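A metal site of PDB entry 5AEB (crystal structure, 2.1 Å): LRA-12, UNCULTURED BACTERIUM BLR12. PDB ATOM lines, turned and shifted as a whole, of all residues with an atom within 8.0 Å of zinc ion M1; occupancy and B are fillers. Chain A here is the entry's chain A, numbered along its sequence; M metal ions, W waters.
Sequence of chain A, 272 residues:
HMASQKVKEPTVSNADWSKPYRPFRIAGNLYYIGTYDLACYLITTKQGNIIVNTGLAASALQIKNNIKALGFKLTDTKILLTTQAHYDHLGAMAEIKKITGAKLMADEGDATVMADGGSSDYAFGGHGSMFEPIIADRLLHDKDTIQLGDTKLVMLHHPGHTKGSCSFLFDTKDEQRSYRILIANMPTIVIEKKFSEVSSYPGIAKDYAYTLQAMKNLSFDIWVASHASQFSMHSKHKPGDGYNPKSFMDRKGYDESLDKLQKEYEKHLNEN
The nearest printed residue that does not touch zinc ion M1 is Asp 88 (4.1 Å).
The side-chain hydroxyl of Thr 188 is in hydrogen-bond range of a ring nitrogen (ND1) of His 161 (2.9 Å).
O of His 161 sits at hydrogen-bond distance from OH of Tyr 122, 3.0 Å away.
The side-chain amide nitrogen (NE2) of Gln 84 lies close to a ring nitrogen (NE2) of His 89 (3.5 Å).
The side-chain amide nitrogen of Gln 84 sits close to the side-chain amide nitrogen of Asn 185 (2.7 Å).
The side-chain carboxylate (OD2) of Asp 121 lies close to a ring nitrogen (NE2) of His 86, 3.3 Å away.
A ring nitrogen (NE2) of His 161 is bound to zinc ion M1, at 1.8 Å.
The side-chain amide oxygen (OE1) of Gln 84 is bound to zinc ion M1 (1.8 Å).
Water W1 is bound to zinc ion M1, 1.9 Å away.
ND1 of His 86 binds zinc ion M1, 1.9 Å away.
Slightly farther from zinc ion M1 lies water W2 (2.7 Å).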
ATOM      1  N   TRP A  17      -1.761  -6.206   5.438  1.00  0.00           N
ATOM      2  CA  TRP A  17      -1.701  -6.848   6.747  1.00  0.00           C
ATOM      3  C   TRP A  17      -3.042  -6.866   7.423  1.00  0.00           C
ATOM      4  O   TRP A  17      -3.387  -7.829   8.067  1.00  0.00           O
ATOM      5  CB  TRP A  17      -0.636  -6.206   7.625  1.00  0.00           C
ATOM      6  CG  TRP A  17       0.776  -6.587   7.256  1.00  0.00           C
ATOM      7  CD1 TRP A  17       1.233  -7.191   6.069  1.00  0.00           C
ATOM      8  CD2 TRP A  17       1.998  -6.397   8.070  1.00  0.00           C
ATOM      9  NE1 TRP A  17       2.589  -7.401   6.124  1.00  0.00           N
ATOM     10  CE2 TRP A  17       3.113  -6.928   7.263  1.00  0.00           C
ATOM     11  CE3 TRP A  17       2.257  -5.837   9.304  1.00  0.00           C
ATOM     12  CZ2 TRP A  17       4.426  -6.908   7.735  1.00  0.00           C
ATOM     13  CZ3 TRP A  17       3.582  -5.843   9.768  1.00  0.00           C
ATOM     14  CH2 TRP A  17       4.645  -6.355   8.992  1.00  0.00           C
ATOM     15  N   THR A  83       4.253 -19.471  14.771  1.00  0.00           N
ATOM     16  CA  THR A  83       5.549 -19.754  14.158  1.00  0.00           C
ATOM     17  C   THR A  83       6.672 -18.774  14.591  1.00  0.00           C
ATOM     18  O   THR A  83       7.852 -18.965  14.201  1.00  0.00           O
ATOM     19  CB  THR A  83       5.412 -19.717  12.649  1.00  0.00           C
ATOM     20  OG1 THR A  83       4.793 -18.474  12.278  1.00  0.00           O
ATOM     21  CG2 THR A  83       4.500 -20.901  12.196  1.00  0.00           C
ATOM     22  N   GLN A  84       6.334 -17.757  15.385  1.00  0.00           N
ATOM     23  CA  GLN A  84       7.142 -16.559  15.375  1.00  0.00           C
ATOM     24  C   GLN A  84       6.606 -15.550  16.383  1.00  0.00           C
ATOM     25  O   GLN A  84       5.480 -15.065  16.201  1.00  0.00           O
ATOM     26  CB  GLN A  84       6.887 -15.903  13.976  1.00  0.00           C
ATOM     27  CG  GLN A  84       8.089 -15.377  13.321  1.00  0.00           C
ATOM     28  CD  GLN A  84       7.738 -14.399  12.247  1.00  0.00           C
ATOM     29  OE1 GLN A  84       7.717 -13.172  12.508  1.00  0.00           O
ATOM     30  NE2 GLN A  84       7.498 -14.924  10.991  1.00  0.00           N
ATOM     31  N   ALA A  85       7.419 -15.112  17.347  1.00  0.00           N
ATOM     32  CA  ALA A  85       6.900 -14.111  18.291  1.00  0.00           C
ATOM     33  C   ALA A  85       7.114 -12.659  17.858  1.00  0.00           C
ATOM     34  O   ALA A  85       7.915 -11.920  18.435  1.00  0.00           O
ATOM     35  CB  ALA A  85       7.455 -14.354  19.699  1.00  0.00           C
ATOM     36  N   HIS A  86       6.406 -12.255  16.808  1.00  0.00           N
ATOM     37  CA  HIS A  86       6.398 -10.872  16.358  1.00  0.00           C
ATOM     38  C   HIS A  86       4.978 -10.426  16.330  1.00  0.00           C
ATOM     39  O   HIS A  86       4.086 -11.227  16.119  1.00  0.00           O
ATOM     40  CB  HIS A  86       6.967 -10.725  14.943  1.00  0.00           C
ATOM     41  CG  HIS A  86       8.476 -10.643  14.882  1.00  0.00           C
ATOM     42  ND1 HIS A  86       9.175 -10.917  13.750  1.00  0.00           N
ATOM     43  CD2 HIS A  86       9.419 -10.326  15.862  1.00  0.00           C
ATOM     44  CE1 HIS A  86      10.492 -10.778  14.008  1.00  0.00           C
ATOM     45  NE2 HIS A  86      10.635 -10.398  15.299  1.00  0.00           N
ATOM     46  N   TYR A  87       4.789  -9.110  16.469  1.00  0.00           N
ATOM     47  CA  TYR A  87       3.461  -8.511  16.605  1.00  0.00           C
ATOM     48  C   TYR A  87       2.546  -8.769  15.411  1.00  0.00           C
ATOM     49  O   TYR A  87       1.326  -8.772  15.586  1.00  0.00           O
ATOM     50  CB  TYR A  87       3.543  -7.001  16.872  1.00  0.00           C
ATOM     51  CG  TYR A  87       3.932  -6.167  15.668  1.00  0.00           C
ATOM     52  CD1 TYR A  87       5.266  -5.977  15.323  1.00  0.00           C
ATOM     53  CD2 TYR A  87       2.949  -5.592  14.855  1.00  0.00           C
ATOM     54  CE1 TYR A  87       5.632  -5.216  14.206  1.00  0.00           C
ATOM     55  CE2 TYR A  87       3.298  -4.837  13.739  1.00  0.00           C
ATOM     56  CZ  TYR A  87       4.626  -4.644  13.415  1.00  0.00           C
ATOM     57  OH  TYR A  87       4.968  -3.886  12.292  1.00  0.00           O
ATOM     58  N   ASP A  88       3.119  -8.968  14.227  1.00  0.00           N
ATOM     59  CA  ASP A  88       2.333  -9.284  13.028  1.00  0.00           C
ATOM     60  C   ASP A  88       1.767 -10.728  13.030  1.00  0.00           C
ATOM     61  O   ASP A  88       0.904 -11.048  12.216  1.00  0.00           O
ATOM     62  CB  ASP A  88       3.080  -8.923  11.680  1.00  0.00           C
ATOM     63  CG  ASP A  88       4.447  -9.600  11.536  1.00  0.00           C
ATOM     64  OD1 ASP A  88       5.193  -9.689  12.566  1.00  0.00           O
ATOM     65  OD2 ASP A  88       4.783 -10.042  10.380  1.00  0.00           O
ATOM     66  N   HIS A  89       2.216 -11.564  13.963  1.00  0.00           N
ATOM     67  CA  HIS A  89       1.690 -12.933  14.111  1.00  0.00           C
ATOM     68  C   HIS A  89       1.158 -13.265  15.470  1.00  0.00           C
ATOM     69  O   HIS A  89       0.629 -14.377  15.664  1.00  0.00           O
ATOM     70  CB  HIS A  89       2.736 -13.950  13.681  1.00  0.00           C
ATOM     71  CG  HIS A  89       3.425 -13.566  12.400  1.00  0.00           C
ATOM     72  ND1 HIS A  89       2.877 -13.787  11.210  1.00  0.00           N
ATOM     73  CD2 HIS A  89       4.634 -12.902  12.167  1.00  0.00           C
ATOM     74  CE1 HIS A  89       3.702 -13.314  10.246  1.00  0.00           C
ATOM     75  NE2 HIS A  89       4.766 -12.765  10.843  1.00  0.00           N
ATOM     76  N   ASP A 121      12.572  -8.155  22.679  1.00  0.00           N
ATOM     77  CA  ASP A 121      12.900  -8.579  21.318  1.00  0.00           C
ATOM     78  C   ASP A 121      14.337  -8.140  20.937  1.00  0.00           C
ATOM     79  O   ASP A 121      14.673  -6.971  21.048  1.00  0.00           O
ATOM     80  CB  ASP A 121      11.871  -8.026  20.309  1.00  0.00           C
ATOM     81  CG  ASP A 121      12.114  -8.507  18.868  1.00  0.00           C
ATOM     82  OD1 ASP A 121      13.226  -8.306  18.341  1.00  0.00           O
ATOM     83  OD2 ASP A 121      11.188  -9.085  18.251  1.00  0.00           O
ATOM     84  N   TYR A 122      15.161  -9.078  20.467  1.00  0.00           N
ATOM     85  CA  TYR A 122      16.559  -8.730  20.110  1.00  0.00           C
ATOM     86  C   TYR A 122      16.661  -7.585  19.085  1.00  0.00           C
ATOM     87  O   TYR A 122      17.618  -6.834  19.110  1.00  0.00           O
ATOM     88  CB  TYR A 122      17.377  -9.953  19.637  1.00  0.00           C
ATOM     89  CG  TYR A 122      17.077 -10.419  18.198  1.00  0.00           C
ATOM     90  CD1 TYR A 122      16.055 -11.345  17.945  1.00  0.00           C
ATOM     91  CD2 TYR A 122      17.816  -9.941  17.118  1.00  0.00           C
ATOM     92  CE1 TYR A 122      15.768 -11.769  16.654  1.00  0.00           C
ATOM     93  CE2 TYR A 122      17.545 -10.360  15.812  1.00  0.00           C
ATOM     94  CZ  TYR A 122      16.518 -11.284  15.580  1.00  0.00           C
ATOM     95  OH  TYR A 122      16.231 -11.708  14.289  1.00  0.00           O
ATOM     96  N   PHE A 124      13.763  -5.435  18.073  1.00  0.00           N
ATOM     97  CA  PHE A 124      12.842  -4.321  18.276  1.00  0.00           C
ATOM     98  C   PHE A 124      12.532  -4.070  19.738  1.00  0.00           C
ATOM     99  O   PHE A 124      11.599  -3.353  20.053  1.00  0.00           O
ATOM    100  CB  PHE A 124      11.552  -4.559  17.516  1.00  0.00           C
ATOM    101  CG  PHE A 124      11.759  -4.805  16.059  1.00  0.00           C
ATOM    102  CD1 PHE A 124      12.317  -3.817  15.249  1.00  0.00           C
ATOM    103  CD2 PHE A 124      11.423  -6.029  15.488  1.00  0.00           C
ATOM    104  CE1 PHE A 124      12.523  -4.037  13.905  1.00  0.00           C
ATOM    105  CE2 PHE A 124      11.618  -6.256  14.138  1.00  0.00           C
ATOM    106  CZ  PHE A 124      12.166  -5.255  13.343  1.00  0.00           C
ATOM    107  N   HIS A 161      15.018 -15.848  12.686  1.00  0.00           N
ATOM    108  CA  HIS A 161      13.995 -14.793  12.548  1.00  0.00           C
ATOM    109  C   HIS A 161      13.609 -14.305  13.931  1.00  0.00           C
ATOM    110  O   HIS A 161      13.577 -13.085  14.171  1.00  0.00           O
ATOM    111  CB  HIS A 161      12.767 -15.255  11.794  1.00  0.00           C
ATOM    112  CG  HIS A 161      11.760 -14.136  11.498  1.00  0.00           C
ATOM    113  ND1 HIS A 161      11.900 -13.303  10.462  1.00  0.00           N
ATOM    114  CD2 HIS A 161      10.612 -13.724  12.181  1.00  0.00           C
ATOM    115  CE1 HIS A 161      10.891 -12.408  10.459  1.00  0.00           C
ATOM    116  NE2 HIS A 161      10.092 -12.674  11.510  1.00  0.00           N
ATOM    117  N   THR A 162      13.309 -15.255  14.828  1.00  0.00           N
ATOM    118  CA  THR A 162      13.210 -14.975  16.245  1.00  0.00           C
ATOM    119  C   THR A 162      14.038 -16.050  16.944  1.00  0.00           C
ATOM    120  O   THR A 162      14.458 -17.049  16.323  1.00  0.00           O
ATOM    121  CB  THR A 162      11.747 -14.879  16.804  1.00  0.00           C
ATOM    122  OG1 THR A 162      11.081 -16.152  16.702  1.00  0.00           O
ATOM    123  CG2 THR A 162      10.968 -13.854  16.081  1.00  0.00           C
ATOM    124  N   SER A 165      11.618 -18.951  16.659  1.00  0.00           N
ATOM    125  CA  SER A 165      10.767 -19.179  15.497  1.00  0.00           C
ATOM    126  C   SER A 165      10.810 -20.663  15.097  1.00  0.00           C
ATOM    127  O   SER A 165      11.818 -21.379  15.352  1.00  0.00           O
ATOM    128  CB  SER A 165      11.032 -18.214  14.332  1.00  0.00           C
ATOM    129  OG  SER A 165      12.413 -17.951  14.140  1.00  0.00           O
ATOM    130  N   ASN A 185       8.134 -21.380   8.976  1.00  0.00           N
ATOM    131  CA  ASN A 185       8.560 -20.017   9.193  1.00  0.00           C
ATOM    132  C   ASN A 185       9.840 -19.757   8.382  1.00  0.00           C
ATOM    133  O   ASN A 185      10.904 -20.225   8.738  1.00  0.00           O
ATOM    134  CB  ASN A 185       8.771 -19.698  10.659  1.00  0.00           C
ATOM    135  CG  ASN A 185       8.796 -18.213  10.871  1.00  0.00           C
ATOM    136  OD1 ASN A 185       9.883 -17.612  10.992  1.00  0.00           O
ATOM    137  ND2 ASN A 185       7.619 -17.589  10.788  1.00  0.00           N
ATOM    138  N   MET A 186       9.723 -19.003   7.287  1.00  0.00           N
ATOM    139  CA  MET A 186      10.893 -18.749   6.396  1.00  0.00           C
ATOM    140  C   MET A 186      11.967 -17.922   7.166  1.00  0.00           C
ATOM    141  O   MET A 186      11.621 -16.979   7.869  1.00  0.00           O
ATOM    142  CB  MET A 186      10.467 -18.038   5.103  1.00  0.00           C
ATOM    143  CG  MET A 186       9.340 -18.761   4.335  1.00  0.00           C
ATOM    144  SD  MET A 186       9.674 -20.524   4.160  1.00  0.00           S
ATOM    145  CE  MET A 186      10.835 -20.514   2.798  1.00  0.00           C
ATOM    146  N   THR A 188      13.802 -15.318   7.155  1.00  0.00           N
ATOM    147  CA  THR A 188      14.100 -14.004   6.692  1.00  0.00           C
ATOM    148  C   THR A 188      14.897 -13.312   7.787  1.00  0.00           C
ATOM    149  O   THR A 188      14.833 -13.701   8.956  1.00  0.00           O
ATOM    150  CB  THR A 188      12.798 -13.258   6.351  1.00  0.00           C
ATOM    151  OG1 THR A 188      11.967 -13.211   7.527  1.00  0.00           O
ATOM    152  CG2 THR A 188      12.035 -13.975   5.184  1.00  0.00           C
ATOM    153  N   VAL A 190      15.717  -9.826   9.806  1.00  0.00           N
ATOM    154  CA  VAL A 190      14.949  -8.687  10.228  1.00  0.00           C
ATOM    155  C   VAL A 190      15.855  -7.475  10.462  1.00  0.00           C
ATOM    156  O   VAL A 190      15.420  -6.333  10.353  1.00  0.00           O
ATOM    157  CB  VAL A 190      14.122  -9.075  11.502  1.00  0.00           C
ATOM    158  CG1 VAL A 190      13.781  -7.885  12.372  1.00  0.00           C
ATOM    159  CG2 VAL A 190      12.864  -9.825  11.094  1.00  0.00           C
ATOM    160  N   SER A 226       4.349 -17.959   7.010  1.00  0.00           N
ATOM    161  CA  SER A 226       3.775 -16.982   7.914  1.00  0.00           C
ATOM    162  C   SER A 226       3.143 -15.776   7.190  1.00  0.00           C
ATOM    163  O   SER A 226       2.229 -15.156   7.703  1.00  0.00           O
ATOM    164  CB  SER A 226       4.830 -16.524   8.916  1.00  0.00           C
ATOM    165  OG  SER A 226       5.072 -17.582   9.868  1.00  0.00           O
ATOM    166  N   HIS A 227       3.639 -15.459   5.995  1.00  0.00           N
ATOM    167  CA  HIS A 227       3.042 -14.396   5.158  1.00  0.00           C
ATOM    168  C   HIS A 227       2.566 -15.008   3.864  1.00  0.00           C
ATOM    169  O   HIS A 227       3.289 -15.817   3.276  1.00  0.00           O
ATOM    170  CB  HIS A 227       4.057 -13.282   4.878  1.00  0.00           C
ATOM    171  CG  HIS A 227       4.353 -12.407   6.078  1.00  0.00           C
ATOM    172  ND1 HIS A 227       3.791 -11.189   6.242  1.00  0.00           N
ATOM    173  CD2 HIS A 227       5.188 -12.611   7.169  1.00  0.00           C
ATOM    174  CE1 HIS A 227       4.205 -10.676   7.435  1.00  0.00           C
ATOM    175  NE2 HIS A 227       5.078 -11.526   7.988  1.00  0.00           N
ATOM    176  N   GLN A 230       4.976 -14.960   1.002  1.00  0.00           N
ATOM    177  CA  GLN A 230       6.175 -15.827   1.024  1.00  0.00           C
ATOM    178  C   GLN A 230       6.007 -17.179   0.356  1.00  0.00           C
ATOM    179  O   GLN A 230       6.976 -17.763  -0.054  1.00  0.00           O
ATOM    180  CB  GLN A 230       6.741 -16.000   2.431  1.00  0.00           C
ATOM    181  CG  GLN A 230       7.125 -14.694   3.083  1.00  0.00           C
ATOM    182  CD  GLN A 230       7.358 -14.840   4.590  1.00  0.00           C
ATOM    183  OE1 GLN A 230       6.661 -15.620   5.304  1.00  0.00           O
ATOM    184  NE2 GLN A 230       8.335 -14.124   5.082  1.00  0.00           N
HETATM  185 ZN    ZN M   1       8.718 -11.727  12.076  1.00  0.00          ZN
HETATM  186 ZN    ZN M   2       5.901 -11.555   9.841  1.00  0.00          ZN
HETATM  187  O   HOH W   1       7.280 -11.037  11.076  1.00  0.00           O
HETATM  188  O   HOH W   2       9.414  -9.508  10.748  1.00  0.00           O
